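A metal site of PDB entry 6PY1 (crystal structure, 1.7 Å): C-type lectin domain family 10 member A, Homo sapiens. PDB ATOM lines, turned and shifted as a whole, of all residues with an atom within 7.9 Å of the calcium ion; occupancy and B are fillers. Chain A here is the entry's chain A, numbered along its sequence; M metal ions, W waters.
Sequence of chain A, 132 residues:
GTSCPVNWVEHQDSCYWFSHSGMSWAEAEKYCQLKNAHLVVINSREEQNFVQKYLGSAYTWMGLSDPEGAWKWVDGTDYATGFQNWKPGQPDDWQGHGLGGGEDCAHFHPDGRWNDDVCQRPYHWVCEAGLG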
ATOM      1  N   HIS A  11       5.385 -15.849 -12.792  1.00  0.00           N
ATOM      2  CA  HIS A  11       6.387 -14.952 -13.422  1.00  0.00           C
ATOM      3  C   HIS A  11       6.073 -14.881 -14.917  1.00  0.00           C
ATOM      4  O   HIS A  11       6.099 -15.935 -15.562  1.00  0.00           O
ATOM      5  CB  HIS A  11       7.814 -15.405 -13.130  1.00  0.00           C
ATOM      6  CG  HIS A  11       8.848 -14.709 -13.952  1.00  0.00           C
ATOM      7  ND1 HIS A  11       9.430 -13.524 -13.538  1.00  0.00           N
ATOM      8  CD2 HIS A  11       9.399 -15.017 -15.145  1.00  0.00           C
ATOM      9  CE1 HIS A  11      10.289 -13.122 -14.450  1.00  0.00           C
ATOM     10  NE2 HIS A  11      10.297 -14.030 -15.453  1.00  0.00           N
ATOM     11  N   GLN A  12       5.760 -13.685 -15.418  1.00  0.00           N
ATOM     12  CA  GLN A  12       5.669 -13.395 -16.875  1.00  0.00           C
ATOM     13  C   GLN A  12       4.823 -14.468 -17.576  1.00  0.00           C
ATOM     14  O   GLN A  12       5.378 -15.179 -18.479  1.00  0.00           O
ATOM     15  CB  GLN A  12       7.044 -13.391 -17.549  1.00  0.00           C
ATOM     16  CG  GLN A  12       8.000 -12.300 -17.085  1.00  0.00           C
ATOM     17  CD  GLN A  12       7.514 -10.917 -17.447  1.00  0.00           C
ATOM     18  OE1 GLN A  12       6.746 -10.729 -18.397  1.00  0.00           O
ATOM     19  NE2 GLN A  12       7.964  -9.934 -16.691  1.00  0.00           N
ATOM     20  N   SER A  14       3.815 -17.428 -16.836  1.00  0.00           N
ATOM     21  CA  SER A  14       3.981 -18.866 -16.472  1.00  0.00           C
ATOM     22  C   SER A  14       3.849 -19.001 -14.966  1.00  0.00           C
ATOM     23  O   SER A  14       4.066 -18.019 -14.256  1.00  0.00           O
ATOM     24  CB  SER A  14       5.349 -19.389 -16.863  1.00  0.00           C
ATOM     25  OG  SER A  14       5.398 -19.767 -18.213  1.00  0.00           O
ATOM     26  N   TYR A  16       5.354 -21.571 -11.882  1.00  0.00           N
ATOM     27  CA  TYR A  16       6.476 -22.478 -11.619  1.00  0.00           C
ATOM     28  C   TYR A  16       6.321 -23.135 -10.268  1.00  0.00           C
ATOM     29  O   TYR A  16       5.786 -22.518  -9.337  1.00  0.00           O
ATOM     30  CB  TYR A  16       7.812 -21.728 -11.649  1.00  0.00           C
ATOM     31  CG  TYR A  16       8.069 -20.981 -12.929  1.00  0.00           C
ATOM     32  CD1 TYR A  16       7.470 -19.771 -13.192  1.00  0.00           C
ATOM     33  CD2 TYR A  16       8.915 -21.498 -13.886  1.00  0.00           C
ATOM     34  CE1 TYR A  16       7.709 -19.095 -14.390  1.00  0.00           C
ATOM     35  CE2 TYR A  16       9.196 -20.817 -15.070  1.00  0.00           C
ATOM     36  CZ  TYR A  16       8.596 -19.605 -15.320  1.00  0.00           C
ATOM     37  OH  TYR A  16       8.853 -18.929 -16.489  1.00  0.00           O
ATOM     38  N   HIS A  38       5.004 -29.082 -17.339  1.00  0.00           N
ATOM     39  CA  HIS A  38       6.155 -29.719 -18.002  1.00  0.00           C
ATOM     40  C   HIS A  38       7.399 -29.287 -17.236  1.00  0.00           C
ATOM     41  O   HIS A  38       7.399 -28.192 -16.615  1.00  0.00           O
ATOM     42  CB  HIS A  38       6.188 -29.352 -19.495  1.00  0.00           C
ATOM     43  CG  HIS A  38       6.267 -27.895 -19.785  1.00  0.00           C
ATOM     44  ND1 HIS A  38       7.458 -27.155 -19.684  1.00  0.00           N
ATOM     45  CD2 HIS A  38       5.304 -27.016 -20.169  1.00  0.00           C
ATOM     46  CE1 HIS A  38       7.223 -25.893 -20.013  1.00  0.00           C
ATOM     47  NE2 HIS A  38       5.874 -25.773 -20.305  1.00  0.00           N
ATOM     48  N   LEU A  39       8.441 -30.075 -17.327  1.00  0.00           N
ATOM     49  CA  LEU A  39       9.766 -29.616 -16.826  1.00  0.00           C
ATOM     50  C   LEU A  39      10.070 -28.263 -17.468  1.00  0.00           C
ATOM     51  O   LEU A  39       9.809 -28.028 -18.649  1.00  0.00           O
ATOM     52  CB  LEU A  39      10.817 -30.659 -17.205  1.00  0.00           C
ATOM     53  CG  LEU A  39      10.935 -31.878 -16.295  1.00  0.00           C
ATOM     54  CD1 LEU A  39      11.898 -32.903 -16.887  1.00  0.00           C
ATOM     55  CD2 LEU A  39      11.356 -31.494 -14.910  1.00  0.00           C
ATOM     56  N   VAL A  40      10.696 -27.380 -16.722  1.00  0.00           N
ATOM     57  CA  VAL A  40      10.850 -25.971 -17.124  1.00  0.00           C
ATOM     58  C   VAL A  40      11.574 -25.911 -18.472  1.00  0.00           C
ATOM     59  O   VAL A  40      12.597 -26.597 -18.669  1.00  0.00           O
ATOM     60  CB  VAL A  40      11.520 -25.149 -16.021  1.00  0.00           C
ATOM     61  CG1 VAL A  40      12.931 -25.650 -15.662  1.00  0.00           C
ATOM     62  CG2 VAL A  40      11.486 -23.662 -16.319  1.00  0.00           C
ATOM     63  N   VAL A  41      11.118 -25.019 -19.340  1.00  0.00           N
ATOM     64  CA  VAL A  41      11.778 -24.672 -20.614  1.00  0.00           C
ATOM     65  C   VAL A  41      12.281 -23.244 -20.485  1.00  0.00           C
ATOM     66  O   VAL A  41      11.431 -22.340 -20.185  1.00  0.00           O
ATOM     67  CB  VAL A  41      10.745 -24.865 -21.747  1.00  0.00           C
ATOM     68  CG1 VAL A  41      11.216 -24.238 -23.038  1.00  0.00           C
ATOM     69  CG2 VAL A  41      10.406 -26.321 -21.935  1.00  0.00           C
ATOM     70  N   ILE A  42      13.589 -23.022 -20.655  1.00  0.00           N
ATOM     71  CA  ILE A  42      14.194 -21.683 -20.542  1.00  0.00           C
ATOM     72  C   ILE A  42      14.163 -21.026 -21.904  1.00  0.00           C
ATOM     73  O   ILE A  42      14.894 -21.478 -22.807  1.00  0.00           O
ATOM     74  CB  ILE A  42      15.576 -21.727 -19.916  1.00  0.00           C
ATOM     75  CG1 ILE A  42      15.514 -22.451 -18.577  1.00  0.00           C
ATOM     76  CG2 ILE A  42      16.148 -20.316 -19.765  1.00  0.00           C
ATOM     77  CD1 ILE A  42      14.625 -21.784 -17.530  1.00  0.00           C
ATOM     78  N   ASN A  43      13.302 -20.016 -22.044  1.00  0.00           N
ATOM     79  CA  ASN A  43      13.027 -19.369 -23.366  1.00  0.00           C
ATOM     80  C   ASN A  43      13.853 -18.113 -23.549  1.00  0.00           C
ATOM     81  O   ASN A  43      13.886 -17.599 -24.697  1.00  0.00           O
ATOM     82  CB  ASN A  43      11.535 -19.063 -23.554  1.00  0.00           C
ATOM     83  CG  ASN A  43      10.690 -20.307 -23.570  1.00  0.00           C
ATOM     84  OD1 ASN A  43      10.416 -20.874 -24.662  1.00  0.00           O
ATOM     85  ND2 ASN A  43      10.298 -20.760 -22.392  1.00  0.00           N
ATOM     86  N   SER A  44      14.505 -17.586 -22.517  1.00  0.00           N
ATOM     87  CA  SER A  44      15.128 -16.233 -22.547  1.00  0.00           C
ATOM     88  C   SER A  44      16.062 -16.043 -21.356  1.00  0.00           C
ATOM     89  O   SER A  44      15.937 -16.780 -20.347  1.00  0.00           O
ATOM     90  CB  SER A  44      14.055 -15.149 -22.553  1.00  0.00           C
ATOM     91  OG  SER A  44      13.363 -15.046 -21.302  1.00  0.00           O
ATOM     92  N   GLU A  47      14.102 -15.206 -18.184  1.00  0.00           N
ATOM     93  CA  GLU A  47      13.550 -16.379 -17.473  1.00  0.00           C
ATOM     94  C   GLU A  47      14.669 -17.170 -16.785  1.00  0.00           C
ATOM     95  O   GLU A  47      14.406 -17.716 -15.702  1.00  0.00           O
ATOM     96  CB  GLU A  47      12.728 -17.230 -18.437  1.00  0.00           C
ATOM     97  CG  GLU A  47      12.172 -18.485 -17.798  1.00  0.00           C
ATOM     98  CD  GLU A  47      11.279 -19.299 -18.728  1.00  0.00           C
ATOM     99  OE1 GLU A  47      10.400 -20.046 -18.203  1.00  0.00           O
ATOM    100  OE2 GLU A  47      11.476 -19.238 -19.969  1.00  0.00           O
ATOM    101  N   GLN A  48      15.806 -17.344 -17.437  1.00  0.00           N
ATOM    102  CA  GLN A  48      17.015 -17.927 -16.821  1.00  0.00           C
ATOM    103  C   GLN A  48      17.302 -17.181 -15.501  1.00  0.00           C
ATOM    104  O   GLN A  48      17.579 -17.841 -14.504  1.00  0.00           O
ATOM    105  CB  GLN A  48      18.197 -17.847 -17.788  1.00  0.00           C
ATOM    106  CG  GLN A  48      19.508 -18.265 -17.143  1.00  0.00           C
ATOM    107  CD  GLN A  48      19.597 -19.731 -16.819  1.00  0.00           C
ATOM    108  OE1 GLN A  48      19.240 -20.586 -17.613  1.00  0.00           O
ATOM    109  NE2 GLN A  48      20.217 -20.028 -15.682  1.00  0.00           N
ATOM    110  N   VAL A  51      14.627 -18.064 -12.755  1.00  0.00           N
ATOM    111  CA  VAL A  51      14.764 -19.466 -12.266  1.00  0.00           C
ATOM    112  C   VAL A  51      16.033 -19.620 -11.439  1.00  0.00           C
ATOM    113  O   VAL A  51      15.986 -20.219 -10.342  1.00  0.00           O
ATOM    114  CB  VAL A  51      14.730 -20.484 -13.423  1.00  0.00           C
ATOM    115  CG1 VAL A  51      15.012 -21.888 -12.894  1.00  0.00           C
ATOM    116  CG2 VAL A  51      13.377 -20.442 -14.099  1.00  0.00           C
ATOM    117  N   TRP A  73      13.827 -29.523 -26.324  1.00  0.00           N
ATOM    118  CA  TRP A  73      12.995 -29.057 -25.187  1.00  0.00           C
ATOM    119  C   TRP A  73      11.716 -29.882 -25.146  1.00  0.00           C
ATOM    120  O   TRP A  73      11.141 -30.200 -26.200  1.00  0.00           O
ATOM    121  CB  TRP A  73      12.721 -27.556 -25.255  1.00  0.00           C
ATOM    122  CG  TRP A  73      13.920 -26.683 -25.057  1.00  0.00           C
ATOM    123  CD1 TRP A  73      14.605 -26.042 -26.032  1.00  0.00           C
ATOM    124  CD2 TRP A  73      14.526 -26.298 -23.823  1.00  0.00           C
ATOM    125  NE1 TRP A  73      15.601 -25.270 -25.490  1.00  0.00           N
ATOM    126  CE2 TRP A  73      15.598 -25.435 -24.140  1.00  0.00           C
ATOM    127  CE3 TRP A  73      14.290 -26.594 -22.481  1.00  0.00           C
ATOM    128  CZ2 TRP A  73      16.407 -24.838 -23.186  1.00  0.00           C
ATOM    129  CZ3 TRP A  73      15.103 -26.014 -21.527  1.00  0.00           C
ATOM    130  CH2 TRP A  73      16.139 -25.151 -21.885  1.00  0.00           C
ATOM    131  N   ASP A  75       8.679 -29.236 -24.695  1.00  0.00           N
ATOM    132  CA  ASP A  75       7.443 -28.639 -25.254  1.00  0.00           C
ATOM    133  C   ASP A  75       7.640 -28.320 -26.732  1.00  0.00           C
ATOM    134  O   ASP A  75       6.707 -27.708 -27.318  1.00  0.00           O
ATOM    135  CB  ASP A  75       7.022 -27.428 -24.429  1.00  0.00           C
ATOM    136  CG  ASP A  75       7.841 -26.176 -24.746  1.00  0.00           C
ATOM    137  OD1 ASP A  75       8.956 -26.284 -25.316  1.00  0.00           O
ATOM    138  OD2 ASP A  75       7.368 -25.093 -24.421  1.00  0.00           O
ATOM    139  N   THR A  77       9.981 -26.217 -28.109  1.00  0.00           N
ATOM    140  CA  THR A  77      10.771 -24.971 -28.325  1.00  0.00           C
ATOM    141  C   THR A  77      12.031 -25.365 -29.084  1.00  0.00           C
ATOM    142  O   THR A  77      12.650 -26.386 -28.728  1.00  0.00           O
ATOM    143  CB  THR A  77      11.092 -24.293 -26.987  1.00  0.00           C
ATOM    144  OG1 THR A  77       9.836 -23.842 -26.473  1.00  0.00           O
ATOM    145  CG2 THR A  77      12.076 -23.156 -27.136  1.00  0.00           C
ATOM    146  N   GLU A 128       6.789 -26.076 -14.969  1.00  0.00           N
ATOM    147  CA  GLU A 128       6.313 -24.814 -15.570  1.00  0.00           C
ATOM    148  C   GLU A 128       4.973 -25.103 -16.253  1.00  0.00           C
ATOM    149  O   GLU A 128       4.859 -26.104 -16.914  1.00  0.00           O
ATOM    150  CB  GLU A 128       7.281 -24.292 -16.606  1.00  0.00           C
ATOM    151  CG  GLU A 128       6.927 -22.917 -17.140  1.00  0.00           C
ATOM    152  CD  GLU A 128       7.840 -22.364 -18.226  1.00  0.00           C
ATOM    153  OE1 GLU A 128       8.762 -23.106 -18.708  1.00  0.00           O
ATOM    154  OE2 GLU A 128       7.581 -21.213 -18.697  1.00  0.00           O
ATOM    155  N   ALA A 129       3.984 -24.255 -15.989  1.00  0.00           N
ATOM    156  CA  ALA A 129       2.665 -24.282 -16.661  1.00  0.00           C
ATOM    157  C   ALA A 129       2.256 -22.870 -17.132  1.00  0.00           C
ATOM    158  O   ALA A 129       2.790 -21.889 -16.647  1.00  0.00           O
ATOM    159  CB  ALA A 129       1.647 -24.878 -15.740  1.00  0.00           C
HETATM  160 CA    CA M   1       9.536 -21.053 -20.241  1.00  0.00          CA
HETATM  161  O   HOH W   1       8.404 -18.957 -20.797  1.00  0.00           O
HETATM  162  O   HOH W   2       8.000 -22.177 -21.552  1.00  0.00           O
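Of the 19 residues printed, 4 come within 4 Å of the calcium ion.
The calcium ion is bound by O of Val 41 (2.3 Å), ND2 of Asn 43 (2.3 Å), water W2 (2.3 Å), OE1 of Glu 47 (2.4 Å), water W1 (2.4 Å), OE2 of Glu 128 (2.5 Å), OE2 of Glu 47 (2.7 Å) and OE1 of Glu 128 (2.7 Å).
The calcium ion has eight donor atoms within binding distance.
The side-chain carboxylate (OE1) of Glu 47 sits close to the side-chain hydroxyl (OH) of Tyr 16.
The side-chain hydroxyl (OG) of Ser 44 is in hydrogen-bond range of the backbone NH (N) of Glu 47, at 3.2 Å.
The side-chain hydroxyl of Tyr 16 lies close to the side-chain carboxylate of Glu 128, at 3.4 Å.
OE2 of Glu 128 sits close to OG of Ser 14 (2.7 Å).
The backbone NH (N) of Glu 128 is in hydrogen-bond range of the backbone carbonyl oxygen (O) of His 38 (2.7 Å).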
